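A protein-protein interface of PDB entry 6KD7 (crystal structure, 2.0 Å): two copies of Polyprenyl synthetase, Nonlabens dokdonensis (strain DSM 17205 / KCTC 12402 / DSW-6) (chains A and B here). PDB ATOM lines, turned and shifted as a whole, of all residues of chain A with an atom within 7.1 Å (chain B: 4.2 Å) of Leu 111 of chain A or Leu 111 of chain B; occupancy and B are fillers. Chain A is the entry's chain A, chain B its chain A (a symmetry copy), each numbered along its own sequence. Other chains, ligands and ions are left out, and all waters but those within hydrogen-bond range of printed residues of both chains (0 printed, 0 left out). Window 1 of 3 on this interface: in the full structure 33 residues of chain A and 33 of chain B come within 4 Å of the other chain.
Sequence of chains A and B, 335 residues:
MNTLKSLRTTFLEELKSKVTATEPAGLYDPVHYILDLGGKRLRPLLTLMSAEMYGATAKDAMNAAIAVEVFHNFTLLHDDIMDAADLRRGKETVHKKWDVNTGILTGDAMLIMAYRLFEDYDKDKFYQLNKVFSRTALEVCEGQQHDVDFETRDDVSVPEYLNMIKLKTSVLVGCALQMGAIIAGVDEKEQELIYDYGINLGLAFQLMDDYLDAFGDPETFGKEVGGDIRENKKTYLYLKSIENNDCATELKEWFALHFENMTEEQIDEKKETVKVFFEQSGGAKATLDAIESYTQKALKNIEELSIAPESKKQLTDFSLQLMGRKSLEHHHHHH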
ATOM      1  N   ALA A  67      26.661 -25.593  -5.746  1.00  0.00           N
ATOM      2  CA  ALA A  67      26.020 -25.472  -7.078  1.00  0.00           C
ATOM      3  C   ALA A  67      26.878 -24.550  -7.954  1.00  0.00           C
ATOM      4  O   ALA A  67      27.071 -24.813  -9.155  1.00  0.00           O
ATOM      5  CB  ALA A  67      24.614 -24.912  -6.998  1.00  0.00           C
ATOM      6  N   VAL A  70      29.994 -26.326  -9.046  1.00  0.00           N
ATOM      7  CA  VAL A  70      29.692 -27.407 -10.012  1.00  0.00           C
ATOM      8  C   VAL A  70      29.376 -26.751 -11.355  1.00  0.00           C
ATOM      9  O   VAL A  70      29.941 -27.180 -12.367  1.00  0.00           O
ATOM     10  CB  VAL A  70      28.586 -28.314  -9.510  1.00  0.00           C
ATOM     11  CG1 VAL A  70      28.123 -29.274 -10.581  1.00  0.00           C
ATOM     12  CG2 VAL A  70      29.082 -29.084  -8.294  1.00  0.00           C
ATOM     13  N   PHE A  71      28.630 -25.656 -11.330  1.00  0.00           N
ATOM     14  CA  PHE A  71      28.249 -24.924 -12.547  1.00  0.00           C
ATOM     15  C   PHE A  71      29.512 -24.440 -13.231  1.00  0.00           C
ATOM     16  O   PHE A  71      29.676 -24.701 -14.435  1.00  0.00           O
ATOM     17  CB  PHE A  71      27.313 -23.740 -12.286  1.00  0.00           C
ATOM     18  CG  PHE A  71      27.097 -22.922 -13.517  1.00  0.00           C
ATOM     19  CD1 PHE A  71      26.282 -23.386 -14.536  1.00  0.00           C
ATOM     20  CD2 PHE A  71      27.766 -21.748 -13.705  1.00  0.00           C
ATOM     21  CE1 PHE A  71      26.141 -22.668 -15.716  1.00  0.00           C
ATOM     22  CE2 PHE A  71      27.628 -21.027 -14.883  1.00  0.00           C
ATOM     23  CZ  PHE A  71      26.818 -21.490 -15.885  1.00  0.00           C
ATOM     24  N   PHE A  74      31.387 -27.054 -14.868  1.00  0.00           N
ATOM     25  CA  PHE A  74      30.666 -27.550 -16.060  1.00  0.00           C
ATOM     26  C   PHE A  74      31.081 -26.674 -17.241  1.00  0.00           C
ATOM     27  O   PHE A  74      31.420 -27.221 -18.270  1.00  0.00           O
ATOM     28  CB  PHE A  74      29.158 -27.464 -15.837  1.00  0.00           C
ATOM     29  CG  PHE A  74      28.362 -26.979 -17.020  1.00  0.00           C
ATOM     30  CD1 PHE A  74      28.147 -27.796 -18.112  1.00  0.00           C
ATOM     31  CD2 PHE A  74      27.805 -25.712 -17.037  1.00  0.00           C
ATOM     32  CE1 PHE A  74      27.400 -27.361 -19.192  1.00  0.00           C
ATOM     33  CE2 PHE A  74      27.057 -25.280 -18.117  1.00  0.00           C
ATOM     34  CZ  PHE A  74      26.863 -26.102 -19.196  1.00  0.00           C
ATOM     35  N   THR A  75      31.140 -25.358 -17.034  1.00  0.00           N
ATOM     36  CA  THR A  75      31.521 -24.447 -18.112  1.00  0.00           C
ATOM     37  C   THR A  75      32.974 -24.731 -18.503  1.00  0.00           C
ATOM     38  O   THR A  75      33.285 -24.608 -19.680  1.00  0.00           O
ATOM     39  CB  THR A  75      31.273 -22.971 -17.798  1.00  0.00           C
ATOM     40  OG1 THR A  75      32.228 -22.493 -16.865  1.00  0.00           O
ATOM     41  CG2 THR A  75      29.869 -22.743 -17.299  1.00  0.00           C
ATOM     42  N   LEU A 105      28.917 -35.211 -22.354  1.00  0.00           N
ATOM     43  CA  LEU A 105      27.864 -35.847 -21.537  1.00  0.00           C
ATOM     44  C   LEU A 105      28.103 -35.558 -20.057  1.00  0.00           C
ATOM     45  O   LEU A 105      27.123 -35.221 -19.370  1.00  0.00           O
ATOM     46  CB  LEU A 105      27.882 -37.349 -21.796  1.00  0.00           C
ATOM     47  CG  LEU A 105      26.807 -38.117 -21.046  1.00  0.00           C
ATOM     48  CD1 LEU A 105      25.422 -37.654 -21.521  1.00  0.00           C
ATOM     49  CD2 LEU A 105      26.975 -39.595 -21.286  1.00  0.00           C
ATOM     50  N   THR A 106      29.342 -35.702 -19.559  1.00  0.00           N
ATOM     51  CA  THR A 106      29.630 -35.414 -18.135  1.00  0.00           C
ATOM     52  C   THR A 106      29.332 -33.948 -17.864  1.00  0.00           C
ATOM     53  O   THR A 106      28.820 -33.631 -16.775  1.00  0.00           O
ATOM     54  CB  THR A 106      31.051 -35.819 -17.750  1.00  0.00           C
ATOM     55  OG1 THR A 106      31.013 -37.240 -17.860  1.00  0.00           O
ATOM     56  CG2 THR A 106      31.410 -35.410 -16.354  1.00  0.00           C
ATOM     57  N   GLY A 107      29.666 -33.048 -18.771  1.00  0.00           N
ATOM     58  CA  GLY A 107      29.381 -31.628 -18.496  1.00  0.00           C
ATOM     59  C   GLY A 107      27.864 -31.406 -18.359  1.00  0.00           C
ATOM     60  O   GLY A 107      27.414 -30.604 -17.500  1.00  0.00           O
ATOM     61  N   ASP A 108      27.082 -32.048 -19.236  1.00  0.00           N
ATOM     62  CA  ASP A 108      25.603 -31.984 -19.194  1.00  0.00           C
ATOM     63  C   ASP A 108      25.145 -32.467 -17.804  1.00  0.00           C
ATOM     64  O   ASP A 108      24.352 -31.769 -17.196  1.00  0.00           O
ATOM     65  CB  ASP A 108      24.980 -32.811 -20.307  1.00  0.00           C
ATOM     66  CG  ASP A 108      25.193 -32.287 -21.722  1.00  0.00           C
ATOM     67  OD1 ASP A 108      25.667 -31.102 -21.885  1.00  0.00           O
ATOM     68  OD2 ASP A 108      24.863 -33.098 -22.688  1.00  0.00           O
ATOM     69  N   ALA A 109      25.663 -33.593 -17.318  1.00  0.00           N
ATOM     70  CA  ALA A 109      25.279 -34.195 -16.024  1.00  0.00           C
ATOM     71  C   ALA A 109      25.636 -33.194 -14.908  1.00  0.00           C
ATOM     72  O   ALA A 109      24.812 -33.013 -13.996  1.00  0.00           O
ATOM     73  CB  ALA A 109      25.883 -35.535 -15.809  1.00  0.00           C
ATOM     74  N   MET A 110      26.732 -32.456 -15.035  1.00  0.00           N
ATOM     75  CA  MET A 110      27.168 -31.528 -13.968  1.00  0.00           C
ATOM     76  C   MET A 110      26.202 -30.349 -13.933  1.00  0.00           C
ATOM     77  O   MET A 110      25.887 -29.899 -12.811  1.00  0.00           O
ATOM     78  CB  MET A 110      28.619 -31.058 -14.153  1.00  0.00           C
ATOM     79  CG  MET A 110      29.616 -32.186 -13.863  1.00  0.00           C
ATOM     80  SD  MET A 110      31.325 -31.626 -14.087  1.00  0.00           S
ATOM     81  CE  MET A 110      31.395 -30.512 -12.696  1.00  0.00           C
ATOM     82  N   LEU A 111      25.792 -29.789 -15.081  1.00  0.00           N
ATOM     83  CA  LEU A 111      24.791 -28.689 -15.047  1.00  0.00           C
ATOM     84  C   LEU A 111      23.523 -29.122 -14.273  1.00  0.00           C
ATOM     85  O   LEU A 111      23.022 -28.359 -13.411  1.00  0.00           O
ATOM     86  CB  LEU A 111      24.448 -28.214 -16.442  1.00  0.00           C
ATOM     87  CG  LEU A 111      23.409 -27.101 -16.530  1.00  0.00           C
ATOM     88  CD1 LEU A 111      23.791 -25.912 -15.642  1.00  0.00           C
ATOM     89  CD2 LEU A 111      23.281 -26.639 -17.985  1.00  0.00           C
ATOM     90  N   ILE A 112      23.084 -30.337 -14.488  1.00  0.00           N
ATOM     91  CA  ILE A 112      21.834 -30.856 -13.882  1.00  0.00           C
ATOM     92  C   ILE A 112      22.089 -31.064 -12.378  1.00  0.00           C
ATOM     93  O   ILE A 112      21.217 -30.722 -11.582  1.00  0.00           O
ATOM     94  CB  ILE A 112      21.384 -32.142 -14.601  1.00  0.00           C
ATOM     95  CG1 ILE A 112      21.040 -31.903 -16.081  1.00  0.00           C
ATOM     96  CG2 ILE A 112      20.206 -32.760 -13.890  1.00  0.00           C
ATOM     97  CD1 ILE A 112      21.083 -33.224 -16.916  1.00  0.00           C
ATOM     98  N   MET A 113      23.246 -31.602 -12.003  1.00  0.00           N
ATOM     99  CA  MET A 113      23.611 -31.821 -10.582  1.00  0.00           C
ATOM    100  C   MET A 113      23.641 -30.474  -9.847  1.00  0.00           C
ATOM    101  O   MET A 113      23.223 -30.413  -8.655  1.00  0.00           O
ATOM    102  CB  MET A 113      24.976 -32.503 -10.499  1.00  0.00           C
ATOM    103  CG  MET A 113      24.948 -33.916 -11.011  1.00  0.00           C
ATOM    104  SD  MET A 113      26.639 -34.559 -11.264  1.00  0.00           S
ATOM    105  CE  MET A 113      27.103 -34.908  -9.574  1.00  0.00           C
ATOM    106  N   ALA A 114      24.097 -29.421 -10.517  1.00  0.00           N
ATOM    107  CA  ALA A 114      24.115 -28.083  -9.922  1.00  0.00           C
ATOM    108  C   ALA A 114      22.677 -27.714  -9.549  1.00  0.00           C
ATOM    109  O   ALA A 114      22.441 -27.270  -8.414  1.00  0.00           O
ATOM    110  CB  ALA A 114      24.703 -27.077 -10.863  1.00  0.00           C
ATOM    111  N   TYR A 115      21.751 -27.815 -10.506  1.00  0.00           N
ATOM    112  CA  TYR A 115      20.332 -27.443 -10.272  1.00  0.00           C
ATOM    113  C   TYR A 115      19.819 -28.229  -9.066  1.00  0.00           C
ATOM    114  O   TYR A 115      19.126 -27.658  -8.260  1.00  0.00           O
ATOM    115  CB  TYR A 115      19.467 -27.701 -11.499  1.00  0.00           C
ATOM    116  CG  TYR A 115      19.493 -26.605 -12.519  1.00  0.00           C
ATOM    117  CD1 TYR A 115      18.703 -25.490 -12.346  1.00  0.00           C
ATOM    118  CD2 TYR A 115      20.209 -26.712 -13.701  1.00  0.00           C
ATOM    119  CE1 TYR A 115      18.688 -24.456 -13.260  1.00  0.00           C
ATOM    120  CE2 TYR A 115      20.180 -25.696 -14.646  1.00  0.00           C
ATOM    121  CZ  TYR A 115      19.399 -24.572 -14.432  1.00  0.00           C
ATOM    122  OH  TYR A 115      19.303 -23.532 -15.293  1.00  0.00           O
ATOM    123  N   ARG A 116      20.161 -29.500  -8.978  1.00  0.00           N
ATOM    124  CA  ARG A 116      19.638 -30.373  -7.903  1.00  0.00           C
ATOM    125  C   ARG A 116      20.105 -29.931  -6.514  1.00  0.00           C
ATOM    126  O   ARG A 116      19.451 -30.294  -5.558  1.00  0.00           O
ATOM    127  CB  ARG A 116      19.986 -31.825  -8.203  1.00  0.00           C
ATOM    128  CG  ARG A 116      19.584 -32.243  -9.604  1.00  0.00           C
ATOM    129  CD  ARG A 116      18.902 -33.575  -9.581  1.00  0.00           C
ATOM    130  NE  ARG A 116      19.692 -34.649  -9.023  1.00  0.00           N
ATOM    131  CZ  ARG A 116      19.149 -35.730  -8.500  1.00  0.00           C
ATOM    132  NH1 ARG A 116      19.909 -36.692  -8.023  1.00  0.00           N
ATOM    133  NH2 ARG A 116      17.841 -35.839  -8.449  1.00  0.00           N
ATOM    134  N   PHE A 133      20.145 -18.041 -11.144  1.00  0.00           N
ATOM    135  CA  PHE A 133      21.114 -19.060 -11.610  1.00  0.00           C
ATOM    136  C   PHE A 133      20.937 -19.290 -13.126  1.00  0.00           C
ATOM    137  O   PHE A 133      21.920 -19.151 -13.873  1.00  0.00           O
ATOM    138  CB  PHE A 133      20.946 -20.365 -10.844  1.00  0.00           C
ATOM    139  CG  PHE A 133      21.894 -21.457 -11.252  1.00  0.00           C
ATOM    140  CD1 PHE A 133      23.242 -21.403 -10.913  1.00  0.00           C
ATOM    141  CD2 PHE A 133      21.430 -22.557 -11.957  1.00  0.00           C
ATOM    142  CE1 PHE A 133      24.090 -22.448 -11.246  1.00  0.00           C
ATOM    143  CE2 PHE A 133      22.296 -23.556 -12.371  1.00  0.00           C
ATOM    144  CZ  PHE A 133      23.616 -23.510 -11.981  1.00  0.00           C
ATOM    145  N   SER A 134      19.705 -19.561 -13.548  1.00  0.00           N
ATOM    146  CA  SER A 134      19.328 -19.824 -14.956  1.00  0.00           C
ATOM    147  C   SER A 134      19.589 -18.595 -15.806  1.00  0.00           C
ATOM    148  O   SER A 134      20.113 -18.724 -16.891  1.00  0.00           O
ATOM    149  CB  SER A 134      17.903 -20.297 -15.074  1.00  0.00           C
ATOM    150  OG  SER A 134      17.760 -21.586 -14.490  1.00  0.00           O
ATOM    151  N   ALA A 137      23.302 -18.505 -16.154  1.00  0.00           N
ATOM    152  CA  ALA A 137      23.852 -19.606 -16.969  1.00  0.00           C
ATOM    153  C   ALA A 137      23.643 -19.257 -18.457  1.00  0.00           C
ATOM    154  O   ALA A 137      24.571 -19.375 -19.256  1.00  0.00           O
ATOM    155  CB  ALA A 137      23.201 -20.886 -16.566  1.00  0.00           C
ATOM    156  N   CYS A 141      26.376 -18.480 -21.637  1.00  0.00           N
ATOM    157  CA  CYS A 141      26.306 -19.044 -23.025  1.00  0.00           C
ATOM    158  C   CYS A 141      26.417 -17.906 -24.057  1.00  0.00           C
ATOM    159  O   CYS A 141      27.204 -18.021 -25.042  1.00  0.00           O
ATOM    160  CB  CYS A 141      25.055 -19.876 -23.256  1.00  0.00           C
ATOM    161  SG  CYS A 141      24.995 -21.366 -22.233  1.00  0.00           S
ATOM    162  N   PHE B  71      13.845 -29.676 -23.908  1.00  0.00           N
ATOM    163  CA  PHE B  71      14.752 -30.622 -23.241  1.00  0.00           C
ATOM    164  C   PHE B  71      15.067 -31.748 -24.207  1.00  0.00           C
ATOM    165  O   PHE B  71      16.257 -32.037 -24.418  1.00  0.00           O
ATOM    166  CB  PHE B  71      14.191 -31.198 -21.937  1.00  0.00           C
ATOM    167  CG  PHE B  71      15.061 -32.282 -21.390  1.00  0.00           C
ATOM    168  CD1 PHE B  71      16.265 -31.975 -20.778  1.00  0.00           C
ATOM    169  CD2 PHE B  71      14.737 -33.595 -21.562  1.00  0.00           C
ATOM    170  CE1 PHE B  71      17.116 -32.982 -20.339  1.00  0.00           C
ATOM    171  CE2 PHE B  71      15.583 -34.604 -21.125  1.00  0.00           C
ATOM    172  CZ  PHE B  71      16.770 -34.294 -20.517  1.00  0.00           C
ATOM    173  N   PHE B  74      17.310 -30.808 -26.875  1.00  0.00           N
ATOM    174  CA  PHE B  74      18.673 -30.573 -26.356  1.00  0.00           C
ATOM    175  C   PHE B  74      19.405 -31.915 -26.373  1.00  0.00           C
ATOM    176  O   PHE B  74      20.515 -31.957 -26.858  1.00  0.00           O
ATOM    177  CB  PHE B  74      18.609 -30.020 -24.933  1.00  0.00           C
ATOM    178  CG  PHE B  74      19.620 -30.592 -23.976  1.00  0.00           C
ATOM    179  CD1 PHE B  74      20.950 -30.228 -24.049  1.00  0.00           C
ATOM    180  CD2 PHE B  74      19.244 -31.480 -22.983  1.00  0.00           C
ATOM    181  CE1 PHE B  74      21.879 -30.738 -23.160  1.00  0.00           C
ATOM    182  CE2 PHE B  74      20.174 -31.986 -22.094  1.00  0.00           C
ATOM    183  CZ  PHE B  74      21.491 -31.620 -22.189  1.00  0.00           C
ATOM    184  N   GLY B 107      23.278 -26.540 -27.413  1.00  0.00           N
ATOM    185  CA  GLY B 107      22.544 -27.546 -26.622  1.00  0.00           C
ATOM    186  C   GLY B 107      22.511 -27.138 -25.138  1.00  0.00           C
ATOM    187  O   GLY B 107      21.479 -27.338 -24.447  1.00  0.00           O
ATOM    188  N   ASP B 108      23.644 -26.639 -24.628  1.00  0.00           N
ATOM    189  CA  ASP B 108      23.751 -26.144 -23.236  1.00  0.00           C
ATOM    190  C   ASP B 108      22.691 -25.045 -23.039  1.00  0.00           C
ATOM    191  O   ASP B 108      21.967 -25.126 -22.061  1.00  0.00           O
ATOM    192  CB  ASP B 108      25.150 -25.634 -22.935  1.00  0.00           C
ATOM    193  CG  ASP B 108      26.247 -26.690 -22.890  1.00  0.00           C
ATOM    194  OD1 ASP B 108      25.918 -27.934 -22.877  1.00  0.00           O
ATOM    195  OD2 ASP B 108      27.472 -26.243 -22.859  1.00  0.00           O
ATOM    196  N   ALA B 109      22.587 -24.086 -23.957  1.00  0.00           N
ATOM    197  CA  ALA B 109      21.649 -22.948 -23.870  1.00  0.00           C
ATOM    198  C   ALA B 109      20.214 -23.510 -23.860  1.00  0.00           C
ATOM    199  O   ALA B 109      19.398 -23.025 -23.057  1.00  0.00           O
ATOM    200  CB  ALA B 109      21.863 -21.940 -24.940  1.00  0.00           C
ATOM    201  N   MET B 110      19.941 -24.583 -24.592  1.00  0.00           N
ATOM    202  CA  MET B 110      18.570 -25.131 -24.681  1.00  0.00           C
ATOM    203  C   MET B 110      18.222 -25.776 -23.344  1.00  0.00           C
ATOM    204  O   MET B 110      17.058 -25.624 -22.919  1.00  0.00           O
ATOM    205  CB  MET B 110      18.405 -26.123 -25.842  1.00  0.00           C
ATOM    206  CG  MET B 110      18.429 -25.411 -27.198  1.00  0.00           C
ATOM    207  SD  MET B 110      18.239 -26.588 -28.563  1.00  0.00           S
ATOM    208  CE  MET B 110      16.542 -27.041 -28.253  1.00  0.00           C
ATOM    209  N   LEU B 111      19.131 -26.538 -22.717  1.00  0.00           N
ATOM    210  CA  LEU B 111      18.817 -27.104 -21.377  1.00  0.00           C
ATOM    211  C   LEU B 111      18.402 -25.986 -20.391  1.00  0.00           C
ATOM    212  O   LEU B 111      17.387 -26.133 -19.667  1.00  0.00           O
ATOM    213  CB  LEU B 111      19.977 -27.912 -20.836  1.00  0.00           C
ATOM    214  CG  LEU B 111      19.777 -28.521 -19.452  1.00  0.00           C
ATOM    215  CD1 LEU B 111      18.483 -29.338 -19.387  1.00  0.00           C
ATOM    216  CD2 LEU B 111      20.972 -29.417 -19.113  1.00  0.00           C
ATOM    217  N   ILE B 112      19.088 -24.872 -20.434  1.00  0.00           N
ATOM    218  CA  ILE B 112      18.858 -23.752 -19.491  1.00  0.00           C
ATOM    219  C   ILE B 112      17.511 -23.100 -19.854  1.00  0.00           C
ATOM    220  O   ILE B 112      16.750 -22.777 -18.944  1.00  0.00           O
ATOM    221  CB  ILE B 112      20.038 -22.762 -19.537  1.00  0.00           C
ATOM    222  CG1 ILE B 112      21.361 -23.399 -19.081  1.00  0.00           C
ATOM    223  CG2 ILE B 112      19.737 -21.543 -18.701  1.00  0.00           C
ATOM    224  CD1 ILE B 112      22.605 -22.601 -19.591  1.00  0.00           C
ATOM    225  N   MET B 113      17.225 -22.915 -21.140  1.00  0.00           N
ATOM    226  CA  MET B 113      15.946 -22.324 -21.606  1.00  0.00           C
ATOM    227  C   MET B 113      14.777 -23.209 -21.150  1.00  0.00           C
ATOM    228  O   MET B 113      13.700 -22.662 -20.778  1.00  0.00           O
ATOM    229  CB  MET B 113      15.959 -22.204 -23.129  1.00  0.00           C
ATOM    230  CG  MET B 113      16.945 -21.180 -23.619  1.00  0.00           C
ATOM    231  SD  MET B 113      17.217 -21.334 -25.418  1.00  0.00           S
ATOM    232  CE  MET B 113      15.725 -20.567 -26.034  1.00  0.00           C
ATOM    233  N   ALA B 114      14.966 -24.525 -21.155  1.00  0.00           N
ATOM    234  CA  ALA B 114      13.931 -25.448 -20.687  1.00  0.00           C
ATOM    235  C   ALA B 114      13.617 -25.105 -19.228  1.00  0.00           C
ATOM    236  O   ALA B 114      12.434 -24.973 -18.879  1.00  0.00           O
ATOM    237  CB  ALA B 114      14.374 -26.874 -20.823  1.00  0.00           C
ATOM    238  N   TYR B 115      14.646 -25.047 -18.378  1.00  0.00           N
ATOM    239  CA  TYR B 115      14.458 -24.766 -16.931  1.00  0.00           C
ATOM    240  C   TYR B 115      13.683 -23.456 -16.791  1.00  0.00           C
ATOM    241  O   TYR B 115      12.810 -23.390 -15.961  1.00  0.00           O
ATOM    242  CB  TYR B 115      15.786 -24.695 -16.189  1.00  0.00           C
ATOM    243  CG  TYR B 115      16.332 -26.024 -15.768  1.00  0.00           C
ATOM    244  CD1 TYR B 115      15.861 -26.626 -14.622  1.00  0.00           C
ATOM    245  CD2 TYR B 115      17.384 -26.635 -16.434  1.00  0.00           C
ATOM    246  CE1 TYR B 115      16.338 -27.847 -14.190  1.00  0.00           C
ATOM    247  CE2 TYR B 115      17.896 -27.848 -15.994  1.00  0.00           C
ATOM    248  CZ  TYR B 115      17.383 -28.446 -14.853  1.00  0.00           C
ATOM    249  OH  TYR B 115      17.816 -29.623 -14.346  1.00  0.00           O
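Of the printed residues of chain B, Leu 111 of chain A touches Leu 111 and Ile 112.
Of the printed residues of chain A, Leu 111 of chain B touches Leu 111 and Ile 112.
Printed residues of chain A within 4 Å of Ile 112 of chain B: Leu 111, Tyr 115, Ser 134, Ala 137 and Cys 141.
Of the printed residues of chain B, Asp 108 of chain A touches Phe 74 and Asp 108.
Of the printed residues of chain A, Tyr 115 of chain B touches Ile 112 and Tyr 115.
Of the printed residues of chain B, Cys 141 of chain A touches Ile 112 (3.8 Å).
Printed residues of chain A within 4 Å of Phe 74 of chain B: Asp 108.
Thr 106 of chain A touches none of the printed residues of chain B.
The nearest printed residue of chain B that does not touch Leu 111 of chain A is Asp 108 of chain B (4.5 Å).
The nearest residue of chain A that does not touch Leu 111 of chain B is Asp 108 of chain A (4.5 Å).
Of the 21 printed residues of chain A, 8 touch a printed residue of chain B.
Hydrophobic or aromatic side chains of chain A within 4 Å of the printed part of chain B: Phe 74, Leu 111, Ile 112, Tyr 115 and Ala 137.
Of the 11 printed residues of chain B, 5 touch a printed residue of chain A.
Hydrophobic or aromatic side chains of chain B that line the printed part of chain A: Phe 74, Leu 111, Ile 112 and Tyr 115.
Along chain B the printed residues that touch a printed residue of chain A span positions 74 to 115.
Among the printed residues, no Asp or Glu carboxylate lies within 4 Å of a Lys or Arg side-chain nitrogen of the other chain.
The side-chain carboxylate of Asp 108 of chain B sits close to the side-chain carboxylate of Asp 108 of chain A, at 3.3 Å.
The side-chain sulfur (SG) of Cys 141 of chain A lies within hydrogen-bond range of the backbone carbonyl oxygen (O) of Ala 137 of chain A (3.6 Å).
The side-chain hydroxyl (OG) of Ser 134 of chain A lies within hydrogen-bond range of the side-chain hydroxyl (OH) of Tyr 115 of chain A, 2.6 Å away.
CZ of Phe 74 of chain A touches OD2 of Asp 108 of chain B, 3.7 Å away.
Asp 108 of chain A touches Phe 74 of chain B (OD2 to CZ, 3.7 Å).
CG1 of Ile 112 of chain B touches CD2 of Leu 111 of chain A, 3.9 Å away.
Ile 112 of chain A touches Leu 111 of chain B.
Tyr 115 of chain B touches Ile 112 of chain A.
Tyr 115 of chain A touches Ile 112 of chain B.
Tyr 115 of chain B touches Tyr 115 of chain A.
Ile 112 of chain B touches Ser 134 of chain A (CG2 to O, 3.4 Å).
Ile 112 of chain B touches Ala 137 of chain A (CD1 to CB, 3.5 Å).
CD1 of Ile 112 of chain B touches SG of Cys 141 of chain A, 3.8 Å away.
Asp 108 of chain B touches its own counterpart, Asp 108 of chain A.
Leu 111 of chain B touches its own counterpart, Leu 111 of chain A.
Leu 111 of chain A touches Ile 112 of chain B, and with the chains exchanged Ile 112 of chain A touches Leu 111 of chain B.
Tyr 115 of chain B touches its own counterpart, Tyr 115 of chain A.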
